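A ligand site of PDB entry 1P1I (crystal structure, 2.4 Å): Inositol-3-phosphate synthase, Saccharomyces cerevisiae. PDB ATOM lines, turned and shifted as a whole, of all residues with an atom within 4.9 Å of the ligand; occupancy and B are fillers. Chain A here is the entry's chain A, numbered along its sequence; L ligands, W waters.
The side-chain carboxylate of Asp 148 lies within hydrogen-bond range of the backbone NH of Gly 74.
The backbone carbonyl oxygen (O) of Asn 355 sits close to the side-chain amide oxygen (OD1) of Asn 246 (3.3 Å).
NE of Arg 198 sits at hydrogen-bond distance from OD1 of Asn 355 (2.7 Å).
The backbone carbonyl oxygen (O) of Ala 245 is in hydrogen-bond range of the indole nitrogen (NE1) of Trp 243, at 3.2 Å.
OG1 of Thr 244 is in hydrogen-bond range of OD1 of Asn 77.
The backbone carbonyl oxygen of Ser 296 sits at hydrogen-bond distance from the backbone NH of Asp 320 (2.7 Å).
The backbone carbonyl oxygen (O) of Arg 198 sits close to the side-chain amide oxygen (OD1) of Asn 150, 3.0 Å away.
The backbone NH of Gly 72 is in hydrogen-bond range of the backbone carbonyl oxygen of Trp 147 (3.1 Å).
Residues that only touch the ligand: Ile 71 (3.6 Å), Gly 72 (3.4 Å), Gly 74 (3.2 Å), Trp 243 (3.8 Å), Thr 244 (3.1 Å), Asn 246 (3.0 Å), Pro 277 (3.99 Å), Gly 295 (3.6 Å), Pro 297 (3.0 Å), Asp 320 (3.2 Å), Leu 321 (3.4 Å), Asn 354 (3.6 Å), Asp 356 (3.5 Å), Asp 438 (3.7 Å), Ser 439 (3.7 Å) and Ala 442 (3.2 Å).
Hydrophobic or aromatic side chains that line the ligand: Ile 71, Ile 149, Trp 243, Ala 245, Pro 277, Pro 297, Leu 321 and Ala 442.
Within 4 Å of the ligand: Ile 71, Gly 72, Gly 74, Gly 75, Asn 76, Asn 77, Asp 148, Ile 149, Ser 184, Ile 185, Arg 198, Trp 243, Thr 244, Ala 245, Asn 246, Thr 247, Pro 277, Gly 295, Ser 296, Pro 297, Asp 320, Leu 321, Asn 354, Asn 355, Asp 356, Asp 438, Ser 439 and Ala 442.
Water W2 lies within hydrogen-bond range of the side-chain hydroxyl (OG) of Ser 439, a nitrogen (N7) of the ligand and the side-chain amide nitrogen (ND2) of Asn 354.
N of Thr 247 sits at hydrogen-bond distance from O12 of the ligand, at 3.0 Å.
An oxygen (O13) of the ligand lies within hydrogen-bond range of the side-chain hydroxyl (OG1) of Thr 247 (2.6 Å).
OD2 of Asp 148 lies within hydrogen-bond range of O6 of the ligand (2.6 Å).
The side-chain hydroxyl of Ser 184 sits at hydrogen-bond distance from a nitrogen (N4) of the ligand, at 2.7 Å.
O1 of the ligand lies close to O of Asn 355 (2.8 Å).
O5 of the ligand lies within hydrogen-bond range of N of Gly 75, at 2.9 Å.
The backbone carbonyl oxygen (O) of Ala 245 is in hydrogen-bond range of an oxygen (O12) of the ligand, at 3.1 Å.
A nitrogen (N3) of the ligand is in hydrogen-bond range of the backbone carbonyl oxygen (O) of Ile 185.
The backbone NH of Asn 77 lies within hydrogen-bond range of an oxygen (O9) of the ligand (3.2 Å).
N7 of the ligand lies close to ND2 of Asn 77, 3.3 Å away.
N of Asn 76 sits at hydrogen-bond distance from O2 of the ligand (3.2 Å).
An oxygen (O2) of the ligand lies within hydrogen-bond range of the side-chain amide nitrogen (ND2) of Asn 76 (3.5 Å).
O6 of the ligand sits at hydrogen-bond distance from NE of Arg 198, at 3.3 Å.
The side-chain hydroxyl (OG) of Ser 296 lies within hydrogen-bond range of an oxygen (O13) of the ligand, at 3.4 Å.
N of Ile 149 lies within hydrogen-bond range of N5 of the ligand, at 3.5 Å.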
ATOM      1  N   ILE A  71      11.727  27.298  -2.648  1.00  0.00           N
ATOM      2  CA  ILE A  71      10.729  26.248  -2.816  1.00  0.00           C
ATOM      3  C   ILE A  71      11.147  25.612  -4.133  1.00  0.00           C
ATOM      4  O   ILE A  71      10.854  26.112  -5.213  1.00  0.00           O
ATOM      5  CB  ILE A  71       9.295  26.835  -2.917  1.00  0.00           C
ATOM      6  CG1 ILE A  71       9.041  27.764  -1.717  1.00  0.00           C
ATOM      7  CG2 ILE A  71       8.270  25.723  -2.935  1.00  0.00           C
ATOM      8  CD1 ILE A  71       7.984  28.781  -1.953  1.00  0.00           C
ATOM      9  N   GLY A  72      11.869  24.500  -4.015  1.00  0.00           N
ATOM     10  CA  GLY A  72      12.363  23.804  -5.180  1.00  0.00           C
ATOM     11  C   GLY A  72      13.846  23.705  -4.941  1.00  0.00           C
ATOM     12  O   GLY A  72      14.640  23.580  -5.869  1.00  0.00           O
ATOM     13  N   GLY A  74      15.700  21.472  -4.235  1.00  0.00           N
ATOM     14  CA  GLY A  74      16.412  20.329  -4.783  1.00  0.00           C
ATOM     15  C   GLY A  74      16.531  20.295  -6.281  1.00  0.00           C
ATOM     16  O   GLY A  74      17.205  19.434  -6.828  1.00  0.00           O
ATOM     17  N   GLY A  75      15.874  21.232  -6.952  1.00  0.00           N
ATOM     18  CA  GLY A  75      15.923  21.281  -8.397  1.00  0.00           C
ATOM     19  C   GLY A  75      17.241  21.789  -8.931  1.00  0.00           C
ATOM     20  O   GLY A  75      18.214  21.969  -8.181  1.00  0.00           O
ATOM     21  N   ASN A  76      17.280  21.998 -10.238  1.00  0.00           N
ATOM     22  CA  ASN A  76      18.481  22.492 -10.901  1.00  0.00           C
ATOM     23  C   ASN A  76      18.867  23.884 -10.372  1.00  0.00           C
ATOM     24  O   ASN A  76      20.015  24.102  -9.967  1.00  0.00           O
ATOM     25  CB  ASN A  76      18.246  22.513 -12.411  1.00  0.00           C
ATOM     26  CG  ASN A  76      17.987  21.112 -12.978  1.00  0.00           C
ATOM     27  OD1 ASN A  76      17.673  20.965 -14.153  1.00  0.00           O
ATOM     28  ND2 ASN A  76      18.123  20.089 -12.140  1.00  0.00           N
ATOM     29  N   ASN A  77      17.915  24.816 -10.361  1.00  0.00           N
ATOM     30  CA  ASN A  77      18.187  26.172  -9.863  1.00  0.00           C
ATOM     31  C   ASN A  77      18.549  26.142  -8.390  1.00  0.00           C
ATOM     32  O   ASN A  77      19.553  26.737  -7.978  1.00  0.00           O
ATOM     33  CB  ASN A  77      16.961  27.067 -10.043  1.00  0.00           C
ATOM     34  CG  ASN A  77      16.604  27.300 -11.490  1.00  0.00           C
ATOM     35  OD1 ASN A  77      15.485  27.731 -11.803  1.00  0.00           O
ATOM     36  ND2 ASN A  77      17.536  27.016 -12.390  1.00  0.00           N
ATOM     37  N   GLY A  78      17.743  25.458  -7.590  1.00  0.00           N
ATOM     38  CA  GLY A  78      17.987  25.395  -6.157  1.00  0.00           C
ATOM     39  C   GLY A  78      19.358  24.881  -5.773  1.00  0.00           C
ATOM     40  O   GLY A  78      20.056  25.493  -4.960  1.00  0.00           O
ATOM     41  N   TRP A 147      12.395  24.331   0.984  1.00  0.00           N
ATOM     42  CA  TRP A 147      11.540  23.148   0.992  1.00  0.00           C
ATOM     43  C   TRP A 147      11.643  22.442  -0.339  1.00  0.00           C
ATOM     44  O   TRP A 147      12.150  23.006  -1.308  1.00  0.00           O
ATOM     45  CB  TRP A 147      10.062  23.533   1.194  1.00  0.00           C
ATOM     46  CG  TRP A 147       9.822  24.400   2.391  1.00  0.00           C
ATOM     47  CD1 TRP A 147       9.577  23.987   3.665  1.00  0.00           C
ATOM     48  CD2 TRP A 147       9.880  25.831   2.427  1.00  0.00           C
ATOM     49  NE1 TRP A 147       9.480  25.069   4.506  1.00  0.00           N
ATOM     50  CE2 TRP A 147       9.662  26.213   3.769  1.00  0.00           C
ATOM     51  CE3 TRP A 147      10.101  26.827   1.467  1.00  0.00           C
ATOM     52  CZ2 TRP A 147       9.658  27.554   4.177  1.00  0.00           C
ATOM     53  CZ3 TRP A 147      10.092  28.170   1.867  1.00  0.00           C
ATOM     54  CH2 TRP A 147       9.877  28.519   3.208  1.00  0.00           C
ATOM     55  N   ASP A 148      11.129  21.221  -0.389  1.00  0.00           N
ATOM     56  CA  ASP A 148      11.108  20.425  -1.609  1.00  0.00           C
ATOM     57  C   ASP A 148      10.369  19.134  -1.320  1.00  0.00           C
ATOM     58  O   ASP A 148      10.584  18.516  -0.269  1.00  0.00           O
ATOM     59  CB  ASP A 148      12.529  20.125  -2.109  1.00  0.00           C
ATOM     60  CG  ASP A 148      12.557  19.740  -3.571  1.00  0.00           C
ATOM     61  OD1 ASP A 148      13.345  20.344  -4.328  1.00  0.00           O
ATOM     62  OD2 ASP A 148      11.792  18.840  -3.974  1.00  0.00           O
ATOM     63  N   ILE A 149       9.505  18.729  -2.236  1.00  0.00           N
ATOM     64  CA  ILE A 149       8.732  17.507  -2.071  1.00  0.00           C
ATOM     65  C   ILE A 149       9.637  16.277  -2.245  1.00  0.00           C
ATOM     66  O   ILE A 149       9.158  15.158  -2.329  1.00  0.00           O
ATOM     67  CB  ILE A 149       7.560  17.429  -3.082  1.00  0.00           C
ATOM     68  CG1 ILE A 149       8.087  17.463  -4.512  1.00  0.00           C
ATOM     69  CG2 ILE A 149       6.581  18.575  -2.835  1.00  0.00           C
ATOM     70  CD1 ILE A 149       7.027  17.233  -5.550  1.00  0.00           C
ATOM     71  N   ASN A 150      10.943  16.500  -2.293  1.00  0.00           N
ATOM     72  CA  ASN A 150      11.909  15.405  -2.410  1.00  0.00           C
ATOM     73  C   ASN A 150      13.041  15.646  -1.409  1.00  0.00           C
ATOM     74  O   ASN A 150      13.525  16.769  -1.255  1.00  0.00           O
ATOM     75  CB  ASN A 150      12.457  15.317  -3.830  1.00  0.00           C
ATOM     76  CG  ASN A 150      13.303  14.080  -4.044  1.00  0.00           C
ATOM     77  OD1 ASN A 150      13.061  13.317  -4.978  1.00  0.00           O
ATOM     78  ND2 ASN A 150      14.288  13.892  -3.191  1.00  0.00           N
ATOM     79  N   SER A 184       7.904  19.557   2.094  1.00  0.00           N
ATOM     80  CA  SER A 184       7.090  20.618   1.537  1.00  0.00           C
ATOM     81  C   SER A 184       5.615  20.255   1.457  1.00  0.00           C
ATOM     82  O   SER A 184       5.189  19.264   2.046  1.00  0.00           O
ATOM     83  CB  SER A 184       7.626  20.964   0.140  1.00  0.00           C
ATOM     84  OG  SER A 184       6.819  21.929  -0.499  1.00  0.00           O
ATOM     85  N   ILE A 185       4.839  21.071   0.742  1.00  0.00           N
ATOM     86  CA  ILE A 185       3.410  20.823   0.555  1.00  0.00           C
ATOM     87  C   ILE A 185       3.241  20.226  -0.841  1.00  0.00           C
ATOM     88  O   ILE A 185       3.821  20.729  -1.810  1.00  0.00           O
ATOM     89  CB  ILE A 185       2.588  22.115   0.631  1.00  0.00           C
ATOM     90  CG1 ILE A 185       2.763  22.772   1.994  1.00  0.00           C
ATOM     91  CG2 ILE A 185       1.133  21.811   0.380  1.00  0.00           C
ATOM     92  CD1 ILE A 185       2.158  24.160   2.099  1.00  0.00           C
ATOM     93  N   ILE A 191       0.189  19.628 -10.640  1.00  0.00           N
ATOM     94  CA  ILE A 191       1.372  19.484 -11.493  1.00  0.00           C
ATOM     95  C   ILE A 191       1.406  18.228 -12.354  1.00  0.00           C
ATOM     96  O   ILE A 191       0.692  17.259 -12.096  1.00  0.00           O
ATOM     97  CB  ILE A 191       2.678  19.498 -10.671  1.00  0.00           C
ATOM     98  CG1 ILE A 191       2.511  18.641  -9.413  1.00  0.00           C
ATOM     99  CG2 ILE A 191       3.098  20.919 -10.364  1.00  0.00           C
ATOM    100  CD1 ILE A 191       3.800  18.443  -8.624  1.00  0.00           C
ATOM    101  N   ARG A 198       8.456  11.173  -7.023  1.00  0.00           N
ATOM    102  CA  ARG A 198       9.486  12.153  -6.682  1.00  0.00           C
ATOM    103  C   ARG A 198       9.172  12.743  -5.305  1.00  0.00           C
ATOM    104  O   ARG A 198      10.063  13.228  -4.605  1.00  0.00           O
ATOM    105  CB  ARG A 198       9.507  13.254  -7.736  1.00  0.00           C
ATOM    106  CG  ARG A 198      10.732  14.160  -7.727  1.00  0.00           C
ATOM    107  CD  ARG A 198      10.591  15.233  -8.807  1.00  0.00           C
ATOM    108  NE  ARG A 198      11.743  16.124  -8.905  1.00  0.00           N
ATOM    109  CZ  ARG A 198      12.960  15.743  -9.281  1.00  0.00           C
ATOM    110  NH1 ARG A 198      13.186  14.468  -9.592  1.00  0.00           N
ATOM    111  NH2 ARG A 198      13.938  16.627  -9.356  1.00  0.00           N
ATOM    112  N   TRP A 243      10.108  31.151  -4.981  1.00  0.00           N
ATOM    113  CA  TRP A 243       9.551  29.943  -5.536  1.00  0.00           C
ATOM    114  C   TRP A 243      10.236  29.550  -6.830  1.00  0.00           C
ATOM    115  O   TRP A 243      10.151  30.290  -7.808  1.00  0.00           O
ATOM    116  CB  TRP A 243       8.056  30.152  -5.805  1.00  0.00           C
ATOM    117  CG  TRP A 243       7.446  29.050  -6.629  1.00  0.00           C
ATOM    118  CD1 TRP A 243       7.554  28.859  -7.980  1.00  0.00           C
ATOM    119  CD2 TRP A 243       6.686  27.930  -6.132  1.00  0.00           C
ATOM    120  NE1 TRP A 243       6.922  27.700  -8.360  1.00  0.00           N
ATOM    121  CE2 TRP A 243       6.385  27.108  -7.241  1.00  0.00           C
ATOM    122  CE3 TRP A 243       6.245  27.539  -4.861  1.00  0.00           C
ATOM    123  CZ2 TRP A 243       5.652  25.922  -7.111  1.00  0.00           C
ATOM    124  CZ3 TRP A 243       5.517  26.366  -4.731  1.00  0.00           C
ATOM    125  CH2 TRP A 243       5.235  25.566  -5.855  1.00  0.00           C
ATOM    126  N   THR A 244      10.899  28.400  -6.833  1.00  0.00           N
ATOM    127  CA  THR A 244      11.561  27.922  -8.047  1.00  0.00           C
ATOM    128  C   THR A 244      11.343  26.417  -8.207  1.00  0.00           C
ATOM    129  O   THR A 244      12.256  25.656  -8.499  1.00  0.00           O
ATOM    130  CB  THR A 244      13.082  28.240  -8.043  1.00  0.00           C
ATOM    131  OG1 THR A 244      13.714  27.599  -9.160  1.00  0.00           O
ATOM    132  CG2 THR A 244      13.735  27.780  -6.758  1.00  0.00           C
ATOM    133  N   ALA A 245      10.093  26.003  -8.024  1.00  0.00           N
ATOM    134  CA  ALA A 245       9.710  24.613  -8.128  1.00  0.00           C
ATOM    135  C   ALA A 245       8.802  24.382  -9.333  1.00  0.00           C
ATOM    136  O   ALA A 245       8.347  25.324  -9.960  1.00  0.00           O
ATOM    137  CB  ALA A 245       9.013  24.193  -6.855  1.00  0.00           C
ATOM    138  N   ASN A 246       8.535  23.121  -9.638  1.00  0.00           N
ATOM    139  CA  ASN A 246       7.673  22.760 -10.755  1.00  0.00           C
ATOM    140  C   ASN A 246       6.468  23.691 -10.876  1.00  0.00           C
ATOM    141  O   ASN A 246       5.889  24.093  -9.874  1.00  0.00           O
ATOM    142  CB  ASN A 246       7.171  21.320 -10.607  1.00  0.00           C
ATOM    143  CG  ASN A 246       8.236  20.292 -10.948  1.00  0.00           C
ATOM    144  OD1 ASN A 246       8.682  20.200 -12.088  1.00  0.00           O
ATOM    145  ND2 ASN A 246       8.633  19.504  -9.968  1.00  0.00           N
ATOM    146  N   THR A 247       6.110  24.021 -12.115  1.00  0.00           N
ATOM    147  CA  THR A 247       4.980  24.887 -12.429  1.00  0.00           C
ATOM    148  C   THR A 247       3.649  24.201 -12.132  1.00  0.00           C
ATOM    149  O   THR A 247       3.357  23.118 -12.652  1.00  0.00           O
ATOM    150  CB  THR A 247       4.952  25.263 -13.919  1.00  0.00           C
ATOM    151  OG1 THR A 247       6.172  25.913 -14.295  1.00  0.00           O
ATOM    152  CG2 THR A 247       3.786  26.186 -14.206  1.00  0.00           C
ATOM    153  N   GLU A 248       2.825  24.837 -11.312  1.00  0.00           N
ATOM    154  CA  GLU A 248       1.517  24.289 -10.986  1.00  0.00           C
ATOM    155  C   GLU A 248       0.588  24.656 -12.134  1.00  0.00           C
ATOM    156  O   GLU A 248       0.963  25.427 -13.012  1.00  0.00           O
ATOM    157  CB  GLU A 248       1.006  24.903  -9.694  1.00  0.00           C
ATOM    158  CG  GLU A 248       2.076  24.992  -8.635  1.00  0.00           C
ATOM    159  CD  GLU A 248       1.574  25.633  -7.376  1.00  0.00           C
ATOM    160  OE1 GLU A 248       0.842  26.639  -7.487  1.00  0.00           O
ATOM    161  OE2 GLU A 248       1.920  25.138  -6.277  1.00  0.00           O
ATOM    162  N   PRO A 277      -0.333  24.977  -3.424  1.00  0.00           N
ATOM    163  CA  PRO A 277       0.826  25.041  -2.540  1.00  0.00           C
ATOM    164  C   PRO A 277       1.466  26.429  -2.520  1.00  0.00           C
ATOM    165  O   PRO A 277       1.673  26.999  -1.449  1.00  0.00           O
ATOM    166  CB  PRO A 277       1.780  23.998  -3.132  1.00  0.00           C
ATOM    167  CG  PRO A 277       0.811  22.952  -3.670  1.00  0.00           C
ATOM    168  CD  PRO A 277      -0.264  23.799  -4.315  1.00  0.00           C
ATOM    169  N   PHE A 281       2.415  28.992   0.290  1.00  0.00           N
ATOM    170  CA  PHE A 281       3.747  29.487   0.550  1.00  0.00           C
ATOM    171  C   PHE A 281       3.724  31.012   0.434  1.00  0.00           C
ATOM    172  O   PHE A 281       4.406  31.713   1.189  1.00  0.00           O
ATOM    173  CB  PHE A 281       4.750  28.915  -0.444  1.00  0.00           C
ATOM    174  CG  PHE A 281       5.287  27.563  -0.037  1.00  0.00           C
ATOM    175  CD1 PHE A 281       4.818  26.406  -0.637  1.00  0.00           C
ATOM    176  CD2 PHE A 281       6.287  27.476   0.923  1.00  0.00           C
ATOM    177  CE1 PHE A 281       5.341  25.174  -0.280  1.00  0.00           C
ATOM    178  CE2 PHE A 281       6.815  26.242   1.288  1.00  0.00           C
ATOM    179  CZ  PHE A 281       6.341  25.088   0.681  1.00  0.00           C
ATOM    180  N   GLY A 295       9.122  32.617  -9.036  1.00  0.00           N
ATOM    181  CA  GLY A 295       9.927  32.334 -10.209  1.00  0.00           C
ATOM    182  C   GLY A 295       9.284  31.446 -11.255  1.00  0.00           C
ATOM    183  O   GLY A 295       9.961  30.992 -12.186  1.00  0.00           O
ATOM    184  N   SER A 296       7.982  31.179 -11.129  1.00  0.00           N
ATOM    185  CA  SER A 296       7.313  30.302 -12.087  1.00  0.00           C
ATOM    186  C   SER A 296       6.153  30.964 -12.791  1.00  0.00           C
ATOM    187  O   SER A 296       5.630  31.982 -12.338  1.00  0.00           O
ATOM    188  CB  SER A 296       6.813  29.036 -11.400  1.00  0.00           C
ATOM    189  OG  SER A 296       7.871  28.138 -11.152  1.00  0.00           O
ATOM    190  N   PRO A 297       5.716  30.370 -13.907  1.00  0.00           N
ATOM    191  CA  PRO A 297       4.603  30.884 -14.707  1.00  0.00           C
ATOM    192  C   PRO A 297       3.183  30.879 -14.125  1.00  0.00           C
ATOM    193  O   PRO A 297       2.375  31.733 -14.490  1.00  0.00           O
ATOM    194  CB  PRO A 297       4.697  30.088 -16.014  1.00  0.00           C
ATOM    195  CG  PRO A 297       5.377  28.813 -15.603  1.00  0.00           C
ATOM    196  CD  PRO A 297       6.407  29.282 -14.617  1.00  0.00           C
ATOM    197  N   ASP A 320       7.248  33.880 -13.469  1.00  0.00           N
ATOM    198  CA  ASP A 320       8.340  33.433 -14.318  1.00  0.00           C
ATOM    199  C   ASP A 320       9.670  34.148 -14.226  1.00  0.00           C
ATOM    200  O   ASP A 320       9.756  35.308 -13.817  1.00  0.00           O
ATOM    201  CB  ASP A 320       7.917  33.422 -15.782  1.00  0.00           C
ATOM    202  CG  ASP A 320       7.892  32.030 -16.368  1.00  0.00           C
ATOM    203  OD1 ASP A 320       8.881  31.280 -16.189  1.00  0.00           O
ATOM    204  OD2 ASP A 320       6.885  31.682 -17.010  1.00  0.00           O
ATOM    205  N   LEU A 321      10.713  33.427 -14.613  1.00  0.00           N
ATOM    206  CA  LEU A 321      12.063  33.952 -14.638  1.00  0.00           C
ATOM    207  C   LEU A 321      12.322  34.205 -16.124  1.00  0.00           C
ATOM    208  O   LEU A 321      12.215  33.298 -16.940  1.00  0.00           O
ATOM    209  CB  LEU A 321      13.051  32.914 -14.088  1.00  0.00           C
ATOM    210  CG  LEU A 321      12.801  32.396 -12.654  1.00  0.00           C
ATOM    211  CD1 LEU A 321      13.834  31.333 -12.301  1.00  0.00           C
ATOM    212  CD2 LEU A 321      12.872  33.530 -11.640  1.00  0.00           C
ATOM    213  N   ASN A 354      16.065  18.149 -18.514  1.00  0.00           N
ATOM    214  CA  ASN A 354      15.901  18.040 -17.071  1.00  0.00           C
ATOM    215  C   ASN A 354      14.443  17.868 -16.639  1.00  0.00           C
ATOM    216  O   ASN A 354      13.585  17.513 -17.461  1.00  0.00           O
ATOM    217  CB  ASN A 354      16.520  19.260 -16.357  1.00  0.00           C
ATOM    218  CG  ASN A 354      15.802  20.559 -16.692  1.00  0.00           C
ATOM    219  OD1 ASN A 354      15.774  20.997 -17.843  1.00  0.00           O
ATOM    220  ND2 ASN A 354      15.235  21.201 -15.670  1.00  0.00           N
ATOM    221  N   ASN A 355      14.179  18.117 -15.350  1.00  0.00           N
ATOM    222  CA  ASN A 355      12.834  17.978 -14.780  1.00  0.00           C
ATOM    223  C   ASN A 355      12.013  19.248 -15.031  1.00  0.00           C
ATOM    224  O   ASN A 355      11.086  19.566 -14.278  1.00  0.00           O
ATOM    225  CB  ASN A 355      12.929  17.711 -13.270  1.00  0.00           C
ATOM    226  CG  ASN A 355      11.628  17.191 -12.677  1.00  0.00           C
ATOM    227  OD1 ASN A 355      11.534  16.926 -11.476  1.00  0.00           O
ATOM    228  ND2 ASN A 355      10.615  17.036 -13.528  1.00  0.00           N
ATOM    229  N   ASP A 356      12.355  19.962 -16.099  1.00  0.00           N
ATOM    230  CA  ASP A 356      11.649  21.177 -16.466  1.00  0.00           C
ATOM    231  C   ASP A 356      11.179  21.039 -17.920  1.00  0.00           C
ATOM    232  O   ASP A 356      11.158  19.937 -18.477  1.00  0.00           O
ATOM    233  CB  ASP A 356      12.585  22.395 -16.331  1.00  0.00           C
ATOM    234  CG  ASP A 356      11.831  23.728 -16.411  1.00  0.00           C
ATOM    235  OD1 ASP A 356      12.507  24.777 -16.540  1.00  0.00           O
ATOM    236  OD2 ASP A 356      10.585  23.728 -16.326  1.00  0.00           O
ATOM    237  N   ASP A 438      20.926  26.107 -19.202  1.00  0.00           N
ATOM    238  CA  ASP A 438      19.831  26.939 -18.716  1.00  0.00           C
ATOM    239  C   ASP A 438      19.905  27.383 -17.256  1.00  0.00           C
ATOM    240  O   ASP A 438      19.899  28.569 -16.954  1.00  0.00           O
ATOM    241  CB  ASP A 438      18.519  26.195 -18.934  1.00  0.00           C
ATOM    242  CG  ASP A 438      17.537  26.991 -19.742  1.00  0.00           C
ATOM    243  OD1 ASP A 438      16.380  26.531 -19.885  1.00  0.00           O
ATOM    244  OD2 ASP A 438      17.927  28.077 -20.210  1.00  0.00           O
ATOM    245  N   SER A 439      19.961  26.415 -16.358  1.00  0.00           N
ATOM    246  CA  SER A 439      20.011  26.697 -14.923  1.00  0.00           C
ATOM    247  C   SER A 439      21.246  27.490 -14.506  1.00  0.00           C
ATOM    248  O   SER A 439      21.367  27.903 -13.354  1.00  0.00           O
ATOM    249  CB  SER A 439      19.960  25.381 -14.133  1.00  0.00           C
ATOM    250  OG  SER A 439      18.830  24.619 -14.516  1.00  0.00           O
ATOM    251  N   ALA A 442      19.863  30.966 -15.132  1.00  0.00           N
ATOM    252  CA  ALA A 442      18.793  31.152 -14.162  1.00  0.00           C
ATOM    253  C   ALA A 442      19.267  31.472 -12.761  1.00  0.00           C
ATOM    254  O   ALA A 442      18.664  32.285 -12.068  1.00  0.00           O
ATOM    255  CB  ALA A 442      17.929  29.917 -14.142  1.00  0.00           C
HETATM  256  P1  LIG L   1      13.439  21.276 -11.515  1.00  0.00           P
HETATM  257  O1  LIG L   1      12.341  20.429 -11.966  1.00  0.00           O
HETATM  258  O2  LIG L   1      14.729  20.551 -11.483  1.00  0.00           O
HETATM  259  O3  LIG L   1      13.284  21.782 -10.039  1.00  0.00           O
HETATM  260  C1  LIG L   1      11.982  21.913  -9.398  1.00  0.00           C
HETATM  261  C2  LIG L   1      12.125  21.449  -7.975  1.00  0.00           C
HETATM  262  O4  LIG L   1      10.855  21.715  -7.344  1.00  0.00           O
HETATM  263  C3  LIG L   1      12.348  19.915  -7.807  1.00  0.00           C
HETATM  264  O5  LIG L   1      13.426  19.686  -6.887  1.00  0.00           O
HETATM  265  C4  LIG L   1      10.963  19.425  -7.301  1.00  0.00           C
HETATM  266  O6  LIG L   1      11.057  18.263  -6.425  1.00  0.00           O
HETATM  267  C5  LIG L   1      10.509  20.652  -6.525  1.00  0.00           C
HETATM  268  N1  LIG L   1       9.071  20.747  -6.329  1.00  0.00           N
HETATM  269  C6  LIG L   1       8.021  20.516  -7.206  1.00  0.00           C
HETATM  270  N2  LIG L   1       6.810  20.892  -6.739  1.00  0.00           N
HETATM  271  C7  LIG L   1       7.142  21.352  -5.453  1.00  0.00           C
HETATM  272  C8  LIG L   1       6.330  21.878  -4.354  1.00  0.00           C
HETATM  273  N3  LIG L   1       4.999  22.013  -4.417  1.00  0.00           N
HETATM  274  N4  LIG L   1       7.002  22.240  -3.191  1.00  0.00           N
HETATM  275  C9  LIG L   1       8.406  22.146  -3.132  1.00  0.00           C
HETATM  276  N5  LIG L   1       9.231  21.673  -4.091  1.00  0.00           N
HETATM  277  C10 LIG L   1       8.539  21.265  -5.210  1.00  0.00           C
HETATM  278  O7  LIG L   1      13.438  22.597 -12.369  1.00  0.00           O
HETATM  279  P2  LIG L   1      14.186  24.033 -12.323  1.00  0.00           P
HETATM  280  O8  LIG L   1      15.059  24.042 -13.537  1.00  0.00           O
HETATM  281  O9  LIG L   1      14.879  24.245 -11.040  1.00  0.00           O
HETATM  282  O10 LIG L   1      12.980  25.047 -12.583  1.00  0.00           O
HETATM  283  C11 LIG L   1      11.954  25.209 -11.587  1.00  0.00           C
HETATM  284  C12 LIG L   1      10.825  26.074 -12.150  1.00  0.00           C
HETATM  285  O11 LIG L   1      11.322  27.411 -12.469  1.00  0.00           O
HETATM  286  C13 LIG L   1      10.067  25.504 -13.342  1.00  0.00           C
HETATM  287  O12 LIG L   1       8.823  24.827 -12.995  1.00  0.00           O
HETATM  288  C14 LIG L   1       9.861  26.733 -14.277  1.00  0.00           C
HETATM  289  O13 LIG L   1       8.479  27.133 -14.360  1.00  0.00           O
HETATM  290  C15 LIG L   1      10.748  27.828 -13.691  1.00  0.00           C
HETATM  291  N6  LIG L   1      11.747  28.392 -14.624  1.00  0.00           N
HETATM  292  C16 LIG L   1      13.038  27.803 -14.645  1.00  0.00           C
HETATM  293  C17 LIG L   1      14.029  28.298 -15.500  1.00  0.00           C
HETATM  294  C18 LIG L   1      15.383  27.584 -15.583  1.00  0.00           C
HETATM  295  O14 LIG L   1      16.288  28.085 -16.223  1.00  0.00           O
HETATM  296  N7  LIG L   1      15.600  26.405 -14.957  1.00  0.00           N
HETATM  297  C19 LIG L   1      13.687  29.399 -16.448  1.00  0.00           C
HETATM  298  C20 LIG L   1      12.330  29.943 -16.464  1.00  0.00           C
HETATM  299  C21 LIG L   1      11.397  29.441 -15.560  1.00  0.00           C
HETATM  300  O   HOH W   1      15.529  24.299  -8.268  1.00  0.00           O
HETATM  301  O   HOH W   2      16.785  24.228 -16.150  1.00  0.00           O
